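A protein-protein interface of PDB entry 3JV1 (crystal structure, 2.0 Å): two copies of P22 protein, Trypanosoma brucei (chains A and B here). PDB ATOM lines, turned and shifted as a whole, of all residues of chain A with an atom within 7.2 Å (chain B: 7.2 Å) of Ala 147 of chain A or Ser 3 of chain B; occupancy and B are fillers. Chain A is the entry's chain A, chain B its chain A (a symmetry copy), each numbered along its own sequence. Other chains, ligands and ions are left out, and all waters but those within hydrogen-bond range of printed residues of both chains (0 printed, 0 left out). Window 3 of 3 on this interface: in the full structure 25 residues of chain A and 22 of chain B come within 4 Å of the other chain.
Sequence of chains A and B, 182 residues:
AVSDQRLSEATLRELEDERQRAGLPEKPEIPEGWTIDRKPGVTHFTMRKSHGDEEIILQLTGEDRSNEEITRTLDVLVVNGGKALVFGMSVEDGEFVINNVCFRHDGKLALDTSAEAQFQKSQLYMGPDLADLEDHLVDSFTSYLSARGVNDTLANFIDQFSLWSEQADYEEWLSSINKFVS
OG of Ser 143 of chain A lies within hydrogen-bond range of NH2 of Arg 6 of chain B, 3.0 Å away.
NH2 of Arg 148 of chain A lies within salt-bridge range of OD1 of Asp 4 of chain B, at 2.7 Å.
The backbone carbonyl oxygen (O) of Tyr 144 of chain A sits at hydrogen-bond distance from the guanidinium group (NH1) of Arg 148 of chain A, 3.0 Å away.
The side-chain amino group of Lys 49 of chain A lies within hydrogen-bond range of the backbone carbonyl oxygen of Arg 148 of chain A, at 3.1 Å.
OD2 of Asp 4 of chain B sits at hydrogen-bond distance from OG of Ser 3 of chain B (2.9 Å).
O of Arg 6 of chain B touches OG of Ser 140 of chain A (3.7 Å).
Ser 140 of chain A touches Leu 7 of chain B (CB to CA, 3.9 Å).
Phe 141 of chain A touches Leu 7 of chain B.
Ser 143 of chain A touches Ser 3 of chain B.
Tyr 144 of chain A touches Ser 3 of chain B (CA to CB, 3.998 Å).
Asp 4 of chain B touches Tyr 144 of chain A (OD2 to CD1, 3.5 Å).
Tyr 144 of chain A touches Leu 7 of chain B (CD1 to CD2, 3.7 Å).
Ser 3 of chain B touches Ala 147 of chain A.
Of the printed residues of chain B, Tyr 144 of chain A touches Ser 3, Asp 4 and Leu 7.
Ser 146 of chain A touches none of the printed residues of chain B.
Ala 147 of chain A touches just one residue of chain B: Ser 3 (3.2 Å).
Val 2 of chain B touches none of the printed residues of chain A.
Of the printed residues of chain A, Ser 3 of chain B touches Ser 143 (3.6 Å), Tyr 144 (3.998 Å) and Ala 147 (3.2 Å).
Of the printed residues of chain A, Asp 4 of chain B touches Tyr 144 and Arg 148.
The nearest residue of chain B that does not touch Ala 147 of chain A is Asp 4 of chain B (5.1 Å).
The nearest printed residue of chain A that does not touch Ser 3 of chain B is Arg 148 of chain A (4.04 Å).
The nearest printed residue of chain B that does not touch Tyr 144 of chain A is Val 181 of chain B (4.1 Å).
Hydrophobic or aromatic side chains of chain A that line the printed part of chain B: Phe 141, Tyr 144 and Ala 147.
Hydrophobic or aromatic side chains of chain B within 4 Å of the printed part of chain A: Leu 7.
Among the printed residues, 10 pairs touch across the chains.
Among the printed residues, Asp or Glu carboxylates within 4 Å of a Lys or Arg side-chain nitrogen of the other chain: Arg 148 of chain A with Asp 4 of chain B.
No position is printed for both chains.
Of the 10 pairs that touch across the chains among the printed residues, none has its exchanged pair printed and touching as well.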
ATOM      1  N   LYS A  49     -15.848   9.191  24.439  1.00  0.00           N
ATOM      2  CA  LYS A  49     -16.298   9.848  23.218  1.00  0.00           C
ATOM      3  C   LYS A  49     -17.611   9.203  22.830  1.00  0.00           C
ATOM      4  O   LYS A  49     -17.854   8.044  23.156  1.00  0.00           O
ATOM      5  CB  LYS A  49     -15.297   9.666  22.073  1.00  0.00           C
ATOM      6  CG  LYS A  49     -15.104   8.221  21.644  1.00  0.00           C
ATOM      7  CD  LYS A  49     -14.460   8.115  20.263  1.00  0.00           C
ATOM      8  CE  LYS A  49     -15.446   8.497  19.166  1.00  0.00           C
ATOM      9  NZ  LYS A  49     -14.909   8.246  17.802  1.00  0.00           N
ATOM     10  N   HIS A  51     -20.402   7.940  19.912  1.00  0.00           N
ATOM     11  CA  HIS A  51     -20.393   7.372  18.572  1.00  0.00           C
ATOM     12  C   HIS A  51     -21.871   7.185  18.269  1.00  0.00           C
ATOM     13  O   HIS A  51     -22.396   6.076  18.339  1.00  0.00           O
ATOM     14  CB  HIS A  51     -19.681   6.018  18.579  1.00  0.00           C
ATOM     15  CG  HIS A  51     -19.552   5.396  17.223  1.00  0.00           C
ATOM     16  ND1 HIS A  51     -18.689   5.876  16.262  1.00  0.00           N
ATOM     17  CD2 HIS A  51     -20.176   4.331  16.667  1.00  0.00           C
ATOM     18  CE1 HIS A  51     -18.787   5.133  15.175  1.00  0.00           C
ATOM     19  NE2 HIS A  51     -19.681   4.189  15.395  1.00  0.00           N
ATOM     20  N   SER A 140     -12.929  -8.834  12.188  1.00  0.00           N
ATOM     21  CA  SER A 140     -14.154  -8.060  12.243  1.00  0.00           C
ATOM     22  C   SER A 140     -14.180  -7.243  13.536  1.00  0.00           C
ATOM     23  O   SER A 140     -14.634  -6.101  13.538  1.00  0.00           O
ATOM     24  CB  SER A 140     -15.362  -8.984  12.158  1.00  0.00           C
ATOM     25  OG  SER A 140     -15.442  -9.568  10.867  1.00  0.00           O
ATOM     26  N   PHE A 141     -13.693  -7.829  14.632  1.00  0.00           N
ATOM     27  CA  PHE A 141     -13.635  -7.115  15.908  1.00  0.00           C
ATOM     28  C   PHE A 141     -12.693  -5.923  15.792  1.00  0.00           C
ATOM     29  O   PHE A 141     -13.029  -4.819  16.226  1.00  0.00           O
ATOM     30  CB  PHE A 141     -13.144  -8.029  17.037  1.00  0.00           C
ATOM     31  CG  PHE A 141     -14.233  -8.825  17.699  1.00  0.00           C
ATOM     32  CD1 PHE A 141     -15.365  -8.194  18.203  1.00  0.00           C
ATOM     33  CD2 PHE A 141     -14.116 -10.202  17.849  1.00  0.00           C
ATOM     34  CE1 PHE A 141     -16.372  -8.919  18.854  1.00  0.00           C
ATOM     35  CE2 PHE A 141     -15.116 -10.942  18.498  1.00  0.00           C
ATOM     36  CZ  PHE A 141     -16.247 -10.294  19.002  1.00  0.00           C
ATOM     37  N   THR A 142     -11.516  -6.141  15.203  1.00  0.00           N
ATOM     38  CA  THR A 142     -10.537  -5.061  15.036  1.00  0.00           C
ATOM     39  C   THR A 142     -11.091  -3.930  14.147  1.00  0.00           C
ATOM     40  O   THR A 142     -10.900  -2.750  14.450  1.00  0.00           O
ATOM     41  CB  THR A 142      -9.183  -5.597  14.471  1.00  0.00           C
ATOM     42  OG1 THR A 142      -8.274  -4.505  14.268  1.00  0.00           O
ATOM     43  CG2 THR A 142      -9.387  -6.287  13.160  1.00  0.00           C
ATOM     44  N   SER A 143     -11.791  -4.284  13.071  1.00  0.00           N
ATOM     45  CA  SER A 143     -12.395  -3.291  12.178  1.00  0.00           C
ATOM     46  C   SER A 143     -13.496  -2.501  12.898  1.00  0.00           C
ATOM     47  O   SER A 143     -13.671  -1.311  12.669  1.00  0.00           O
ATOM     48  CB  SER A 143     -13.000  -3.979  10.954  1.00  0.00           C
ATOM     49  OG  SER A 143     -12.010  -4.706  10.259  1.00  0.00           O
ATOM     50  N   TYR A 144     -14.254  -3.187  13.748  1.00  0.00           N
ATOM     51  CA  TYR A 144     -15.318  -2.569  14.535  1.00  0.00           C
ATOM     52  C   TYR A 144     -14.704  -1.495  15.460  1.00  0.00           C
ATOM     53  O   TYR A 144     -15.228  -0.388  15.591  1.00  0.00           O
ATOM     54  CB  TYR A 144     -16.015  -3.656  15.362  1.00  0.00           C
ATOM     55  CG  TYR A 144     -17.095  -3.178  16.300  1.00  0.00           C
ATOM     56  CD1 TYR A 144     -18.404  -2.988  15.855  1.00  0.00           C
ATOM     57  CD2 TYR A 144     -16.822  -2.970  17.653  1.00  0.00           C
ATOM     58  CE1 TYR A 144     -19.414  -2.613  16.737  1.00  0.00           C
ATOM     59  CE2 TYR A 144     -17.819  -2.596  18.539  1.00  0.00           C
ATOM     60  CZ  TYR A 144     -19.109  -2.421  18.082  1.00  0.00           C
ATOM     61  OH  TYR A 144     -20.094  -2.064  18.973  1.00  0.00           O
ATOM     62  N   LEU A 145     -13.588  -1.829  16.096  1.00  0.00           N
ATOM     63  CA  LEU A 145     -12.917  -0.888  16.982  1.00  0.00           C
ATOM     64  C   LEU A 145     -12.307   0.266  16.190  1.00  0.00           C
ATOM     65  O   LEU A 145     -12.353   1.420  16.616  1.00  0.00           O
ATOM     66  CB  LEU A 145     -11.824  -1.600  17.773  1.00  0.00           C
ATOM     67  CG  LEU A 145     -12.324  -2.599  18.811  1.00  0.00           C
ATOM     68  CD1 LEU A 145     -11.167  -3.428  19.301  1.00  0.00           C
ATOM     69  CD2 LEU A 145     -12.991  -1.849  19.963  1.00  0.00           C
ATOM     70  N   SER A 146     -11.741  -0.048  15.031  1.00  0.00           N
ATOM     71  CA  SER A 146     -11.131   0.975  14.204  1.00  0.00           C
ATOM     72  C   SER A 146     -12.160   1.993  13.700  1.00  0.00           C
ATOM     73  O   SER A 146     -11.877   3.181  13.638  1.00  0.00           O
ATOM     74  CB  SER A 146     -10.405   0.335  13.024  1.00  0.00           C
ATOM     75  OG  SER A 146      -9.588   1.295  12.384  1.00  0.00           O
ATOM     76  N   ALA A 147     -13.354   1.533  13.349  1.00  0.00           N
ATOM     77  CA  ALA A 147     -14.397   2.438  12.870  1.00  0.00           C
ATOM     78  C   ALA A 147     -14.815   3.417  13.963  1.00  0.00           C
ATOM     79  O   ALA A 147     -15.442   4.441  13.686  1.00  0.00           O
ATOM     80  CB  ALA A 147     -15.610   1.648  12.393  1.00  0.00           C
ATOM     81  N   ARG A 148     -14.470   3.098  15.208  1.00  0.00           N
ATOM     82  CA  ARG A 148     -14.812   3.955  16.326  1.00  0.00           C
ATOM     83  C   ARG A 148     -13.616   4.761  16.843  1.00  0.00           C
ATOM     84  O   ARG A 148     -13.673   5.353  17.920  1.00  0.00           O
ATOM     85  CB  ARG A 148     -15.434   3.110  17.446  1.00  0.00           C
ATOM     86  CG  ARG A 148     -16.780   2.520  17.030  1.00  0.00           C
ATOM     87  CD  ARG A 148     -17.288   1.412  17.946  1.00  0.00           C
ATOM     88  NE  ARG A 148     -18.664   1.085  17.590  1.00  0.00           N
ATOM     89  CZ  ARG A 148     -19.034   0.636  16.393  1.00  0.00           C
ATOM     90  NH1 ARG A 148     -18.125   0.441  15.446  1.00  0.00           N
ATOM     91  NH2 ARG A 148     -20.314   0.445  16.118  1.00  0.00           N
ATOM     92  N   GLY A 149     -12.535   4.792  16.072  1.00  0.00           N
ATOM     93  CA  GLY A 149     -11.369   5.553  16.492  1.00  0.00           C
ATOM     94  C   GLY A 149     -10.362   4.820  17.356  1.00  0.00           C
ATOM     95  O   GLY A 149      -9.312   5.370  17.685  1.00  0.00           O
ATOM     96  N   VAL A 150     -10.664   3.583  17.737  1.00  0.00           N
ATOM     97  CA  VAL A 150      -9.732   2.814  18.555  1.00  0.00           C
ATOM     98  C   VAL A 150      -8.768   2.155  17.587  1.00  0.00           C
ATOM     99  O   VAL A 150      -8.940   1.001  17.188  1.00  0.00           O
ATOM    100  CB  VAL A 150     -10.462   1.752  19.389  1.00  0.00           C
ATOM    101  CG1 VAL A 150      -9.488   1.087  20.341  1.00  0.00           C
ATOM    102  CG2 VAL A 150     -11.604   2.404  20.163  1.00  0.00           C
ATOM    103  N   ASN A 151      -7.751   2.924  17.213  1.00  0.00           N
ATOM    104  CA  ASN A 151      -6.751   2.499  16.251  1.00  0.00           C
ATOM    105  C   ASN A 151      -5.340   2.807  16.744  1.00  0.00           C
ATOM    106  O   ASN A 151      -5.146   3.155  17.909  1.00  0.00           O
ATOM    107  CB  ASN A 151      -7.032   3.211  14.925  1.00  0.00           C
ATOM    108  CG  ASN A 151      -7.357   4.685  15.121  1.00  0.00           C
ATOM    109  OD1 ASN A 151      -8.088   5.289  14.332  1.00  0.00           O
ATOM    110  ND2 ASN A 151      -6.807   5.273  16.173  1.00  0.00           N
ATOM    111  N   ALA B   1     -20.808   1.606  10.099  1.00  0.00           N
ATOM    112  CA  ALA B   1     -21.927   0.935   9.376  1.00  0.00           C
ATOM    113  C   ALA B   1     -21.464  -0.392   8.780  1.00  0.00           C
ATOM    114  O   ALA B   1     -21.968  -1.454   9.143  1.00  0.00           O
ATOM    115  CB  ALA B   1     -22.460   1.848   8.271  1.00  0.00           C
ATOM    116  N   VAL B   2     -20.502  -0.323   7.866  1.00  0.00           N
ATOM    117  CA  VAL B   2     -19.974  -1.524   7.223  1.00  0.00           C
ATOM    118  C   VAL B   2     -19.267  -2.450   8.217  1.00  0.00           C
ATOM    119  O   VAL B   2     -19.500  -3.659   8.219  1.00  0.00           O
ATOM    120  CB  VAL B   2     -18.995  -1.154   6.090  1.00  0.00           C
ATOM    121  CG1 VAL B   2     -18.427  -2.420   5.454  1.00  0.00           C
ATOM    122  CG2 VAL B   2     -19.718  -0.313   5.042  1.00  0.00           C
ATOM    123  N   SER B   3     -18.410  -1.883   9.060  1.00  0.00           N
ATOM    124  CA  SER B   3     -17.686  -2.671  10.055  1.00  0.00           C
ATOM    125  C   SER B   3     -18.666  -3.417  10.963  1.00  0.00           C
ATOM    126  O   SER B   3     -18.437  -4.569  11.326  1.00  0.00           O
ATOM    127  CB  SER B   3     -16.794  -1.761  10.908  1.00  0.00           C
ATOM    128  OG  SER B   3     -17.571  -0.835  11.653  1.00  0.00           O
ATOM    129  N   ASP B   4     -19.758  -2.751  11.325  1.00  0.00           N
ATOM    130  CA  ASP B   4     -20.771  -3.350  12.181  1.00  0.00           C
ATOM    131  C   ASP B   4     -21.506  -4.464  11.441  1.00  0.00           C
ATOM    132  O   ASP B   4     -21.924  -5.454  12.041  1.00  0.00           O
ATOM    133  CB  ASP B   4     -21.769  -2.291  12.640  1.00  0.00           C
ATOM    134  CG  ASP B   4     -21.102  -1.132  13.376  1.00  0.00           C
ATOM    135  OD1 ASP B   4     -21.833  -0.321  13.977  1.00  0.00           O
ATOM    136  OD2 ASP B   4     -19.857  -1.023  13.350  1.00  0.00           O
ATOM    137  N   GLN B   5     -21.668  -4.293  10.134  1.00  0.00           N
ATOM    138  CA  GLN B   5     -22.339  -5.295   9.322  1.00  0.00           C
ATOM    139  C   GLN B   5     -21.427  -6.527   9.251  1.00  0.00           C
ATOM    140  O   GLN B   5     -21.889  -7.657   9.368  1.00  0.00           O
ATOM    141  CB  GLN B   5     -22.616  -4.719   7.929  1.00  0.00           C
ATOM    142  CG  GLN B   5     -23.546  -5.552   7.067  1.00  0.00           C
ATOM    143  CD  GLN B   5     -24.088  -4.774   5.877  1.00  0.00           C
ATOM    144  OE1 GLN B   5     -24.705  -5.345   4.978  1.00  0.00           O
ATOM    145  NE2 GLN B   5     -23.866  -3.463   5.872  1.00  0.00           N
ATOM    146  N   ARG B   6     -20.129  -6.290   9.076  1.00  0.00           N
ATOM    147  CA  ARG B   6     -19.133  -7.356   9.026  1.00  0.00           C
ATOM    148  C   ARG B   6     -19.118  -8.151  10.333  1.00  0.00           C
ATOM    149  O   ARG B   6     -19.074  -9.379  10.316  1.00  0.00           O
ATOM    150  CB  ARG B   6     -17.741  -6.778   8.803  1.00  0.00           C
ATOM    151  CG  ARG B   6     -17.475  -6.270   7.402  1.00  0.00           C
ATOM    152  CD  ARG B   6     -16.105  -5.601   7.325  1.00  0.00           C
ATOM    153  NE  ARG B   6     -15.063  -6.413   7.952  1.00  0.00           N
ATOM    154  CZ  ARG B   6     -13.765  -6.130   7.902  1.00  0.00           C
ATOM    155  NH1 ARG B   6     -13.341  -5.049   7.253  1.00  0.00           N
ATOM    156  NH2 ARG B   6     -12.889  -6.930   8.499  1.00  0.00           N
ATOM    157  N   LEU B   7     -19.147  -7.443  11.464  1.00  0.00           N
ATOM    158  CA  LEU B   7     -19.129  -8.100  12.770  1.00  0.00           C
ATOM    159  C   LEU B   7     -20.416  -8.878  12.985  1.00  0.00           C
ATOM    160  O   LEU B   7     -20.416  -9.950  13.598  1.00  0.00           O
ATOM    161  CB  LEU B   7     -18.936  -7.076  13.900  1.00  0.00           C
ATOM    162  CG  LEU B   7     -18.837  -7.687  15.306  1.00  0.00           C
ATOM    163  CD1 LEU B   7     -17.831  -8.840  15.298  1.00  0.00           C
ATOM    164  CD2 LEU B   7     -18.417  -6.621  16.314  1.00  0.00           C
ATOM    165  N   SER B   8     -21.518  -8.331  12.479  1.00  0.00           N
ATOM    166  CA  SER B   8     -22.814  -8.993  12.589  1.00  0.00           C
ATOM    167  C   SER B   8     -22.780 -10.316  11.818  1.00  0.00           C
ATOM    168  O   SER B   8     -23.201 -11.354  12.324  1.00  0.00           O
ATOM    169  CB  SER B   8     -23.916  -8.097  12.016  1.00  0.00           C
ATOM    170  OG  SER B   8     -25.166  -8.760  12.055  1.00  0.00           O
ATOM    171  N   GLU B   9     -22.267 -10.272  10.592  1.00  0.00           N
ATOM    172  CA  GLU B   9     -22.171 -11.464   9.748  1.00  0.00           C
ATOM    173  C   GLU B   9     -21.195 -12.493  10.316  1.00  0.00           C
ATOM    174  O   GLU B   9     -21.474 -13.691  10.322  1.00  0.00           O
ATOM    175  CB  GLU B   9     -21.712 -11.082   8.340  1.00  0.00           C
ATOM    176  CG  GLU B   9     -22.701 -10.259   7.541  1.00  0.00           C
ATOM    177  CD  GLU B   9     -22.119  -9.791   6.212  1.00  0.00           C
ATOM    178  OE1 GLU B   9     -21.688 -10.652   5.416  1.00  0.00           O
ATOM    179  OE2 GLU B   9     -22.089  -8.566   5.962  1.00  0.00           O
ATOM    180  N   VAL B 181     -24.582  -5.675  17.853  1.00  0.00           N
ATOM    181  CA  VAL B 181     -24.037  -5.021  16.672  1.00  0.00           C
ATOM    182  C   VAL B 181     -25.085  -4.835  15.572  1.00  0.00           C
ATOM    183  O   VAL B 181     -24.833  -4.181  14.560  1.00  0.00           O
ATOM    184  CB  VAL B 181     -22.832  -5.820  16.137  1.00  0.00           C
ATOM    185  CG1 VAL B 181     -22.254  -5.148  14.910  1.00  0.00           C
ATOM    186  CG2 VAL B 181     -21.768  -5.909  17.226  1.00  0.00           C
